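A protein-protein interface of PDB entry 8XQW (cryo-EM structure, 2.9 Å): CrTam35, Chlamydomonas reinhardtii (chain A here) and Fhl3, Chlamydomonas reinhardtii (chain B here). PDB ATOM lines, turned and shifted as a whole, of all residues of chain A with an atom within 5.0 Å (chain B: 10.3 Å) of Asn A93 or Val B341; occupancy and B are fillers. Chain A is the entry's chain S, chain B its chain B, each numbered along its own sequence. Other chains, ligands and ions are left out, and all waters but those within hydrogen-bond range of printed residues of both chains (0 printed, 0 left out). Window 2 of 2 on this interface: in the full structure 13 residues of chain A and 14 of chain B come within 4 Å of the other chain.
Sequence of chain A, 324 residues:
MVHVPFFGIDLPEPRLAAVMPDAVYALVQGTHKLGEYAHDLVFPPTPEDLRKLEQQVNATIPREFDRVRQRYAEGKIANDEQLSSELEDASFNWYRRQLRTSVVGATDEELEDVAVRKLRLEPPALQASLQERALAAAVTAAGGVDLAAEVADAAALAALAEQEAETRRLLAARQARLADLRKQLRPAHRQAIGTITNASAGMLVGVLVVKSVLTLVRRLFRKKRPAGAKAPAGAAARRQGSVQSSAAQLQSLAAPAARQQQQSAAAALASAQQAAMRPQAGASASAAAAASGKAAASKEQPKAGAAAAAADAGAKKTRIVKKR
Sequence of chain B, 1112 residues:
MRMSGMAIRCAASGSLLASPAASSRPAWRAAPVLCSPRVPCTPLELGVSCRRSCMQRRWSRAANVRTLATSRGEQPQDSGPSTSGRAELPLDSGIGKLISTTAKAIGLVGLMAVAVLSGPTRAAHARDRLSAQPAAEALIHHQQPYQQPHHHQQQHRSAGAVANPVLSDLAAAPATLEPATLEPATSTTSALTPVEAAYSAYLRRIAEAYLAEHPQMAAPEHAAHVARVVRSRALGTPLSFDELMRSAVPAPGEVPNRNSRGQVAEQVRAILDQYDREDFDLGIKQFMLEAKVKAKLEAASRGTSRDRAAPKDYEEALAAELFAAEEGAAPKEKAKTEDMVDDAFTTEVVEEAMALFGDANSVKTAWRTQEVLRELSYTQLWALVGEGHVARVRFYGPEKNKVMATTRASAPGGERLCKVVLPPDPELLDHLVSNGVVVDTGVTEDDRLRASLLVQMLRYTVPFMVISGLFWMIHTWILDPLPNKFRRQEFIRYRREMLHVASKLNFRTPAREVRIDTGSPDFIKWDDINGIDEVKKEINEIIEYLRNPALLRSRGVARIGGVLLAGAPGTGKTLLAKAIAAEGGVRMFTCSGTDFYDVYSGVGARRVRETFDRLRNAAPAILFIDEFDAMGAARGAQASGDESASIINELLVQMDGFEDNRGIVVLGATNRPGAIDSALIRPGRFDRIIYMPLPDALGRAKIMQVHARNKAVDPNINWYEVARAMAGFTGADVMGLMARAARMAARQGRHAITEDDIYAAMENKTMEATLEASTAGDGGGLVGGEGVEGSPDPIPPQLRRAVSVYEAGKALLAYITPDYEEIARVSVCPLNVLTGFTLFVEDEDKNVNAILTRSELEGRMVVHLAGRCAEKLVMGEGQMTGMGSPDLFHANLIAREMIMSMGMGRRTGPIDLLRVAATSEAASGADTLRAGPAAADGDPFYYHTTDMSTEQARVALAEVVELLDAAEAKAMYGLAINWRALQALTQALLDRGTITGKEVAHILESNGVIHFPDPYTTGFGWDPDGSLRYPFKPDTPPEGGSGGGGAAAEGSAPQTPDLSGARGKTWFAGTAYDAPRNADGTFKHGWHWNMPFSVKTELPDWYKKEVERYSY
O2P of TPO B347 lies close to the guanidinium group (NH1) of Arg A96, 3.5 Å away. The backbone carbonyl oxygen (O) of Asp B343 lies within hydrogen-bond range of the guanidinium group (NE) of Arg A96 (2.8 Å).
The backbone carbonyl oxygen (O) of Asp A89 lies close to the side-chain amide oxygen (OD1) of Asn A93 (2.8 Å). OE2 of Glu A64 is in salt-bridge range of NE of Arg A97. The side-chain amide oxygen of Asn A93 lies within hydrogen-bond range of the guanidinium group of Arg A96. The backbone carbonyl oxygen of Phe A92 is in hydrogen-bond range of the guanidinium group of Arg A96 (3.5 Å).
TPO B347 touches Phe A92. Asn A93 touches Val B341. Phe B345 touches Arg A96. Arg A97 touches Asp B343.
Of chain B, only Val B341 (3.4 Å) comes within 4 Å of Asn A93. Of the printed residues of chain B, Arg A96 touches Asp B343 (2.8 Å), Phe B345 (3.7 Å) and TPO B347 (3.5 Å). Of the printed residues of chain B, Arg A97 touches Asp B343 (3.7 Å). Printed residues of chain A within 4 Å of TPO B347: Phe A92 and Arg A96. Of the printed residues of chain B, Phe A92 touches TPO B347. Printed residues of chain A within 4 Å of Asp B343: Arg A96 (2.8 Å) and Arg A97 (3.7 Å). TPO B346 touches none of the printed residues of chain A. The nearest printed residue of chain B that does not touch Phe A92 is Asp B343 (6.3 Å).
Of the 13 printed residues of chain B, 4 touch a printed residue of chain A. Printed residues of chain B that touch a printed residue of chain A: Val B341, Asp B343, Phe B345 and TPO B347. Hydrophobic or aromatic side chains of chain B that line the printed part of chain A: Val B341 and Phe B345. Among the printed residues, no Asp or Glu carboxylate lies within 4 Å of a Lys or Arg side-chain nitrogen of the other chain.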
ATOM      1  N   GLU A  64     -14.557  -8.989  -9.349  1.00  0.00           N
ATOM      2  CA  GLU A  64     -15.693  -9.388 -10.176  1.00  0.00           C
ATOM      3  C   GLU A  64     -15.270 -10.085 -11.459  1.00  0.00           C
ATOM      4  O   GLU A  64     -16.125 -10.627 -12.167  1.00  0.00           O
ATOM      5  CB  GLU A  64     -16.547  -8.169 -10.528  1.00  0.00           C
ATOM      6  CG  GLU A  64     -17.819  -8.030  -9.717  1.00  0.00           C
ATOM      7  CD  GLU A  64     -17.552  -7.671  -8.272  1.00  0.00           C
ATOM      8  OE1 GLU A  64     -18.475  -7.819  -7.446  1.00  0.00           O
ATOM      9  OE2 GLU A  64     -16.421  -7.238  -7.961  1.00  0.00           O
ATOM     10  N   GLU A  88     -18.752  -7.949 -20.265  1.00  0.00           N
ATOM     11  CA  GLU A  88     -19.710  -6.884 -19.987  1.00  0.00           C
ATOM     12  C   GLU A  88     -20.466  -7.136 -18.691  1.00  0.00           C
ATOM     13  O   GLU A  88     -20.756  -6.194 -17.946  1.00  0.00           O
ATOM     14  CB  GLU A  88     -20.691  -6.736 -21.145  1.00  0.00           C
ATOM     15  CG  GLU A  88     -20.044  -6.325 -22.451  1.00  0.00           C
ATOM     16  CD  GLU A  88     -21.044  -5.805 -23.463  1.00  0.00           C
ATOM     17  OE1 GLU A  88     -20.633  -5.039 -24.358  1.00  0.00           O
ATOM     18  OE2 GLU A  88     -22.238  -6.159 -23.368  1.00  0.00           O
ATOM     19  N   ASP A  89     -20.789  -8.396 -18.400  1.00  0.00           N
ATOM     20  CA  ASP A  89     -21.542  -8.701 -17.187  1.00  0.00           C
ATOM     21  C   ASP A  89     -20.714  -8.414 -15.941  1.00  0.00           C
ATOM     22  O   ASP A  89     -21.177  -7.735 -15.017  1.00  0.00           O
ATOM     23  CB  ASP A  89     -21.990 -10.157 -17.206  1.00  0.00           C
ATOM     24  CG  ASP A  89     -22.292 -10.648 -18.602  1.00  0.00           C
ATOM     25  OD1 ASP A  89     -23.331 -10.246 -19.166  1.00  0.00           O
ATOM     26  OD2 ASP A  89     -21.487 -11.436 -19.138  1.00  0.00           O
ATOM     27  N   ALA A  90     -19.490  -8.940 -15.893  1.00  0.00           N
ATOM     28  CA  ALA A  90     -18.601  -8.617 -14.788  1.00  0.00           C
ATOM     29  C   ALA A  90     -18.381  -7.116 -14.691  1.00  0.00           C
ATOM     30  O   ALA A  90     -18.337  -6.555 -13.588  1.00  0.00           O
ATOM     31  CB  ALA A  90     -17.271  -9.344 -14.956  1.00  0.00           C
ATOM     32  N   SER A  91     -18.260  -6.448 -15.837  1.00  0.00           N
ATOM     33  CA  SER A  91     -18.015  -5.013 -15.834  1.00  0.00           C
ATOM     34  C   SER A  91     -19.163  -4.265 -15.183  1.00  0.00           C
ATOM     35  O   SER A  91     -18.945  -3.396 -14.337  1.00  0.00           O
ATOM     36  CB  SER A  91     -17.813  -4.511 -17.256  1.00  0.00           C
ATOM     37  OG  SER A  91     -19.062  -4.170 -17.824  1.00  0.00           O
ATOM     38  N   PHE A  92     -20.396  -4.579 -15.573  1.00  0.00           N
ATOM     39  CA  PHE A  92     -21.529  -3.859 -15.010  1.00  0.00           C
ATOM     40  C   PHE A  92     -21.768  -4.239 -13.559  1.00  0.00           C
ATOM     41  O   PHE A  92     -22.260  -3.417 -12.781  1.00  0.00           O
ATOM     42  CB  PHE A  92     -22.775  -4.102 -15.845  1.00  0.00           C
ATOM     43  CG  PHE A  92     -22.870  -3.219 -17.046  1.00  0.00           C
ATOM     44  CD1 PHE A  92     -22.190  -3.532 -18.206  1.00  0.00           C
ATOM     45  CD2 PHE A  92     -23.628  -2.069 -17.017  1.00  0.00           C
ATOM     46  CE1 PHE A  92     -22.276  -2.721 -19.315  1.00  0.00           C
ATOM     47  CE2 PHE A  92     -23.715  -1.254 -18.123  1.00  0.00           C
ATOM     48  CZ  PHE A  92     -23.039  -1.582 -19.273  1.00  0.00           C
ATOM     49  N   ASN A  93     -21.416  -5.461 -13.164  1.00  0.00           N
ATOM     50  CA  ASN A  93     -21.479  -5.801 -11.747  1.00  0.00           C
ATOM     51  C   ASN A  93     -20.522  -4.932 -10.943  1.00  0.00           C
ATOM     52  O   ASN A  93     -20.893  -4.370  -9.903  1.00  0.00           O
ATOM     53  CB  ASN A  93     -21.165  -7.281 -11.552  1.00  0.00           C
ATOM     54  CG  ASN A  93     -22.273  -8.178 -12.052  1.00  0.00           C
ATOM     55  OD1 ASN A  93     -23.041  -7.803 -12.937  1.00  0.00           O
ATOM     56  ND2 ASN A  93     -22.370  -9.370 -11.480  1.00  0.00           N
ATOM     57  N   TRP A  94     -19.284  -4.797 -11.422  1.00  0.00           N
ATOM     58  CA  TRP A  94     -18.329  -3.912 -10.765  1.00  0.00           C
ATOM     59  C   TRP A  94     -18.818  -2.472 -10.766  1.00  0.00           C
ATOM     60  O   TRP A  94     -18.659  -1.749  -9.778  1.00  0.00           O
ATOM     61  CB  TRP A  94     -16.973  -4.012 -11.455  1.00  0.00           C
ATOM     62  CG  TRP A  94     -15.918  -3.253 -10.751  1.00  0.00           C
ATOM     63  CD1 TRP A  94     -15.295  -3.604  -9.596  1.00  0.00           C
ATOM     64  CD2 TRP A  94     -15.357  -2.000 -11.146  1.00  0.00           C
ATOM     65  NE1 TRP A  94     -14.376  -2.651  -9.245  1.00  0.00           N
ATOM     66  CE2 TRP A  94     -14.396  -1.654 -10.183  1.00  0.00           C
ATOM     67  CE3 TRP A  94     -15.571  -1.140 -12.223  1.00  0.00           C
ATOM     68  CZ2 TRP A  94     -13.651  -0.486 -10.264  1.00  0.00           C
ATOM     69  CZ3 TRP A  94     -14.834   0.016 -12.301  1.00  0.00           C
ATOM     70  CH2 TRP A  94     -13.886   0.335 -11.330  1.00  0.00           C
ATOM     71  N   TYR A  95     -19.425  -2.045 -11.869  1.00  0.00           N
ATOM     72  CA  TYR A  95     -19.915  -0.678 -11.990  1.00  0.00           C
ATOM     73  C   TYR A  95     -21.001  -0.383 -10.965  1.00  0.00           C
ATOM     74  O   TYR A  95     -20.972   0.658 -10.297  1.00  0.00           O
ATOM     75  CB  TYR A  95     -20.426  -0.465 -13.411  1.00  0.00           C
ATOM     76  CG  TYR A  95     -20.965   0.902 -13.717  1.00  0.00           C
ATOM     77  CD1 TYR A  95     -20.366   2.037 -13.209  1.00  0.00           C
ATOM     78  CD2 TYR A  95     -22.061   1.060 -14.543  1.00  0.00           C
ATOM     79  CE1 TYR A  95     -20.855   3.287 -13.499  1.00  0.00           C
ATOM     80  CE2 TYR A  95     -22.555   2.305 -14.840  1.00  0.00           C
ATOM     81  CZ  TYR A  95     -21.946   3.414 -14.316  1.00  0.00           C
ATOM     82  OH  TYR A  95     -22.436   4.660 -14.607  1.00  0.00           O
ATOM     83  N   ARG A  96     -21.959  -1.294 -10.810  1.00  0.00           N
ATOM     84  CA  ARG A  96     -23.027  -1.060  -9.846  1.00  0.00           C
ATOM     85  C   ARG A  96     -22.513  -1.170  -8.417  1.00  0.00           C
ATOM     86  O   ARG A  96     -22.982  -0.452  -7.523  1.00  0.00           O
ATOM     87  CB  ARG A  96     -24.179  -2.026 -10.096  1.00  0.00           C
ATOM     88  CG  ARG A  96     -24.951  -1.717 -11.365  1.00  0.00           C
ATOM     89  CD  ARG A  96     -26.200  -2.565 -11.490  1.00  0.00           C
ATOM     90  NE  ARG A  96     -25.937  -3.972 -11.214  1.00  0.00           N
ATOM     91  CZ  ARG A  96     -25.608  -4.865 -12.138  1.00  0.00           C
ATOM     92  NH1 ARG A  96     -25.507  -4.502 -13.407  1.00  0.00           N
ATOM     93  NH2 ARG A  96     -25.388  -6.122 -11.791  1.00  0.00           N
ATOM     94  N   ARG A  97     -21.531  -2.043  -8.179  1.00  0.00           N
ATOM     95  CA  ARG A  97     -20.903  -2.059  -6.865  1.00  0.00           C
ATOM     96  C   ARG A  97     -20.249  -0.723  -6.560  1.00  0.00           C
ATOM     97  O   ARG A  97     -20.324  -0.231  -5.429  1.00  0.00           O
ATOM     98  CB  ARG A  97     -19.872  -3.176  -6.772  1.00  0.00           C
ATOM     99  CG  ARG A  97     -19.280  -3.305  -5.389  1.00  0.00           C
ATOM    100  CD  ARG A  97     -18.459  -4.558  -5.269  1.00  0.00           C
ATOM    101  NE  ARG A  97     -17.302  -4.526  -6.149  1.00  0.00           N
ATOM    102  CZ  ARG A  97     -16.059  -4.341  -5.727  1.00  0.00           C
ATOM    103  NH1 ARG A  97     -15.818  -4.174  -4.437  1.00  0.00           N
ATOM    104  NH2 ARG A  97     -15.061  -4.324  -6.593  1.00  0.00           N
ATOM    105  N   ALA B 335     -27.722 -18.809 -16.879  1.00  0.00           N
ATOM    106  CA  ALA B 335     -27.550 -18.128 -15.603  1.00  0.00           C
ATOM    107  C   ALA B 335     -28.891 -17.965 -14.902  1.00  0.00           C
ATOM    108  O   ALA B 335     -29.905 -17.681 -15.541  1.00  0.00           O
ATOM    109  CB  ALA B 335     -26.898 -16.763 -15.822  1.00  0.00           C
ATOM    110  N   LYS B 336     -28.895 -18.150 -13.587  1.00  0.00           N
ATOM    111  CA  LYS B 336     -30.110 -17.942 -12.802  1.00  0.00           C
ATOM    112  C   LYS B 336     -29.792 -17.597 -11.349  1.00  0.00           C
ATOM    113  O   LYS B 336     -28.626 -17.522 -10.960  1.00  0.00           O
ATOM    114  CB  LYS B 336     -31.046 -19.163 -12.862  1.00  0.00           C
ATOM    115  CG  LYS B 336     -30.427 -20.528 -12.569  1.00  0.00           C
ATOM    116  CD  LYS B 336     -29.683 -21.102 -13.762  1.00  0.00           C
ATOM    117  CE  LYS B 336     -29.098 -22.469 -13.454  1.00  0.00           C
ATOM    118  NZ  LYS B 336     -28.155 -22.899 -14.524  1.00  0.00           N
ATOM    119  N   TPO B 337     -30.851 -17.390 -10.565  1.00  0.00           N
ATOM    120  CA  TPO B 337     -30.770 -16.804  -9.226  1.00  0.00           C
ATOM    121  CB  TPO B 337     -32.173 -16.581  -8.683  1.00  0.00           C
ATOM    122  CG2 TPO B 337     -32.232 -15.242  -7.947  1.00  0.00           C
ATOM    123  OG1 TPO B 337     -33.079 -16.537  -9.784  1.00  0.00           O
ATOM    124  P   TPO B 337     -33.994 -17.856  -9.724  1.00  0.00           P
ATOM    125  O1P TPO B 337     -33.713 -18.640  -8.347  1.00  0.00           O
ATOM    126  O2P TPO B 337     -33.638 -18.798 -10.977  1.00  0.00           O
ATOM    127  O3P TPO B 337     -35.418 -17.461  -9.788  1.00  0.00           O
ATOM    128  C   TPO B 337     -29.946 -17.637  -8.247  1.00  0.00           C
ATOM    129  O   TPO B 337     -29.623 -18.788  -8.529  1.00  0.00           O
ATOM    130  N   GLU B 338     -29.599 -17.032  -7.109  1.00  0.00           N
ATOM    131  CA  GLU B 338     -28.587 -17.567  -6.185  1.00  0.00           C
ATOM    132  C   GLU B 338     -27.229 -17.768  -6.859  1.00  0.00           C
ATOM    133  O   GLU B 338     -26.431 -18.609  -6.453  1.00  0.00           O
ATOM    134  CB  GLU B 338     -29.054 -18.873  -5.532  1.00  0.00           C
ATOM    135  CG  GLU B 338     -30.242 -18.734  -4.588  1.00  0.00           C
ATOM    136  CD  GLU B 338     -31.566 -18.545  -5.291  1.00  0.00           C
ATOM    137  OE1 GLU B 338     -31.874 -17.398  -5.667  1.00  0.00           O
ATOM    138  OE2 GLU B 338     -32.302 -19.538  -5.452  1.00  0.00           O
ATOM    139  N   ASP B 339     -26.993 -16.987  -7.908  1.00  0.00           N
ATOM    140  CA  ASP B 339     -25.678 -16.833  -8.502  1.00  0.00           C
ATOM    141  C   ASP B 339     -25.387 -15.378  -8.827  1.00  0.00           C
ATOM    142  O   ASP B 339     -24.251 -15.057  -9.188  1.00  0.00           O
ATOM    143  CB  ASP B 339     -25.546 -17.685  -9.772  1.00  0.00           C
ATOM    144  CG  ASP B 339     -25.851 -19.149  -9.525  1.00  0.00           C
ATOM    145  OD1 ASP B 339     -27.034 -19.495  -9.345  1.00  0.00           O
ATOM    146  OD2 ASP B 339     -24.900 -19.955  -9.499  1.00  0.00           O
ATOM    147  N   MET B 340     -26.379 -14.499  -8.730  1.00  0.00           N
ATOM    148  CA  MET B 340     -26.172 -13.071  -8.871  1.00  0.00           C
ATOM    149  C   MET B 340     -25.652 -12.486  -7.562  1.00  0.00           C
ATOM    150  O   MET B 340     -25.992 -12.941  -6.467  1.00  0.00           O
ATOM    151  CB  MET B 340     -27.475 -12.378  -9.266  1.00  0.00           C
ATOM    152  CG  MET B 340     -28.259 -13.088 -10.351  1.00  0.00           C
ATOM    153  SD  MET B 340     -27.283 -13.359 -11.836  1.00  0.00           S
ATOM    154  CE  MET B 340     -28.482 -12.962 -13.100  1.00  0.00           C
ATOM    155  N   VAL B 341     -24.810 -11.466  -7.689  1.00  0.00           N
ATOM    156  CA  VAL B 341     -24.285 -10.768  -6.524  1.00  0.00           C
ATOM    157  C   VAL B 341     -25.249  -9.653  -6.124  1.00  0.00           C
ATOM    158  O   VAL B 341     -25.910  -9.036  -6.962  1.00  0.00           O
ATOM    159  CB  VAL B 341     -22.873 -10.229  -6.820  1.00  0.00           C
ATOM    160  CG1 VAL B 341     -22.879  -9.445  -8.118  1.00  0.00           C
ATOM    161  CG2 VAL B 341     -22.336  -9.404  -5.667  1.00  0.00           C
ATOM    162  N   ASP B 342     -25.326  -9.385  -4.825  1.00  0.00           N
ATOM    163  CA  ASP B 342     -26.429  -8.593  -4.275  1.00  0.00           C
ATOM    164  C   ASP B 342     -26.277  -7.101  -4.560  1.00  0.00           C
ATOM    165  O   ASP B 342     -26.261  -6.269  -3.659  1.00  0.00           O
ATOM    166  CB  ASP B 342     -26.548  -8.854  -2.781  1.00  0.00           C
ATOM    167  CG  ASP B 342     -26.725 -10.321  -2.463  1.00  0.00           C
ATOM    168  OD1 ASP B 342     -26.225 -11.157  -3.242  1.00  0.00           O
ATOM    169  OD2 ASP B 342     -27.370 -10.638  -1.442  1.00  0.00           O
ATOM    170  N   ASP B 343     -26.171  -6.760  -5.839  1.00  0.00           N
ATOM    171  CA  ASP B 343     -26.233  -5.381  -6.309  1.00  0.00           C
ATOM    172  C   ASP B 343     -27.080  -5.332  -7.575  1.00  0.00           C
ATOM    173  O   ASP B 343     -26.714  -4.727  -8.584  1.00  0.00           O
ATOM    174  CB  ASP B 343     -24.834  -4.816  -6.537  1.00  0.00           C
ATOM    175  CG  ASP B 343     -24.238  -4.233  -5.277  1.00  0.00           C
ATOM    176  OD1 ASP B 343     -24.964  -3.514  -4.562  1.00  0.00           O
ATOM    177  OD2 ASP B 343     -23.049  -4.490  -4.996  1.00  0.00           O
ATOM    178  N   ALA B 344     -28.234  -5.996  -7.527  1.00  0.00           N
ATOM    179  CA  ALA B 344     -29.021  -6.301  -8.711  1.00  0.00           C
ATOM    180  C   ALA B 344     -30.161  -5.320  -8.948  1.00  0.00           C
ATOM    181  O   ALA B 344     -31.221  -5.722  -9.440  1.00  0.00           O
ATOM    182  CB  ALA B 344     -29.560  -7.727  -8.615  1.00  0.00           C
ATOM    183  N   PHE B 345     -29.985  -4.050  -8.614  1.00  0.00           N
ATOM    184  CA  PHE B 345     -31.003  -3.061  -8.930  1.00  0.00           C
ATOM    185  C   PHE B 345     -30.952  -2.739 -10.415  1.00  0.00           C
ATOM    186  O   PHE B 345     -29.971  -3.051 -11.085  1.00  0.00           O
ATOM    187  CB  PHE B 345     -30.809  -1.794  -8.104  1.00  0.00           C
ATOM    188  CG  PHE B 345     -29.380  -1.369  -7.982  1.00  0.00           C
ATOM    189  CD1 PHE B 345     -28.783  -0.621  -8.979  1.00  0.00           C
ATOM    190  CD2 PHE B 345     -28.633  -1.717  -6.877  1.00  0.00           C
ATOM    191  CE1 PHE B 345     -27.466  -0.233  -8.874  1.00  0.00           C
ATOM    192  CE2 PHE B 345     -27.318  -1.329  -6.769  1.00  0.00           C
ATOM    193  CZ  PHE B 345     -26.735  -0.585  -7.768  1.00  0.00           C
ATOM    194  N   TPO B 346     -32.016  -2.131 -10.929  1.00  0.00           N
ATOM    195  CA  TPO B 346     -32.037  -1.674 -12.311  1.00  0.00           C
ATOM    196  CB  TPO B 346     -33.442  -1.274 -12.725  1.00  0.00           C
ATOM    197  CG2 TPO B 346     -33.424  -0.726 -14.153  1.00  0.00           C
ATOM    198  OG1 TPO B 346     -34.289  -2.422 -12.654  1.00  0.00           O
ATOM    199  P   TPO B 346     -35.541  -2.054 -11.711  1.00  0.00           P
ATOM    200  O1P TPO B 346     -35.039  -1.774 -10.209  1.00  0.00           O
ATOM    201  O2P TPO B 346     -36.503  -3.174 -11.699  1.00  0.00           O
ATOM    202  O3P TPO B 346     -36.282  -0.749 -12.283  1.00  0.00           O
ATOM    203  C   TPO B 346     -31.073  -0.511 -12.454  1.00  0.00           C
ATOM    204  O   TPO B 346     -31.168   0.466 -11.717  1.00  0.00           O
ATOM    205  N   TPO B 347     -30.144  -0.623 -13.397  1.00  0.00           N
ATOM    206  CA  TPO B 347     -29.006   0.289 -13.468  1.00  0.00           C
ATOM    207  CB  TPO B 347     -27.970  -0.250 -14.432  1.00  0.00           C
ATOM    208  CG2 TPO B 347     -26.598   0.288 -14.034  1.00  0.00           C
ATOM    209  OG1 TPO B 347     -27.952  -1.673 -14.395  1.00  0.00           O
ATOM    210  P   TPO B 347     -27.987  -2.129 -15.933  1.00  0.00           P
ATOM    211  O1P TPO B 347     -29.344  -2.945 -16.204  1.00  0.00           O
ATOM    212  O2P TPO B 347     -26.817  -2.978 -16.235  1.00  0.00           O
ATOM    213  O3P TPO B 347     -27.951  -0.819 -16.862  1.00  0.00           O
ATOM    214  C   TPO B 347     -29.375   1.711 -13.864  1.00  0.00           C
ATOM    215  O   TPO B 347     -29.044   2.655 -13.159  1.00  0.00           O
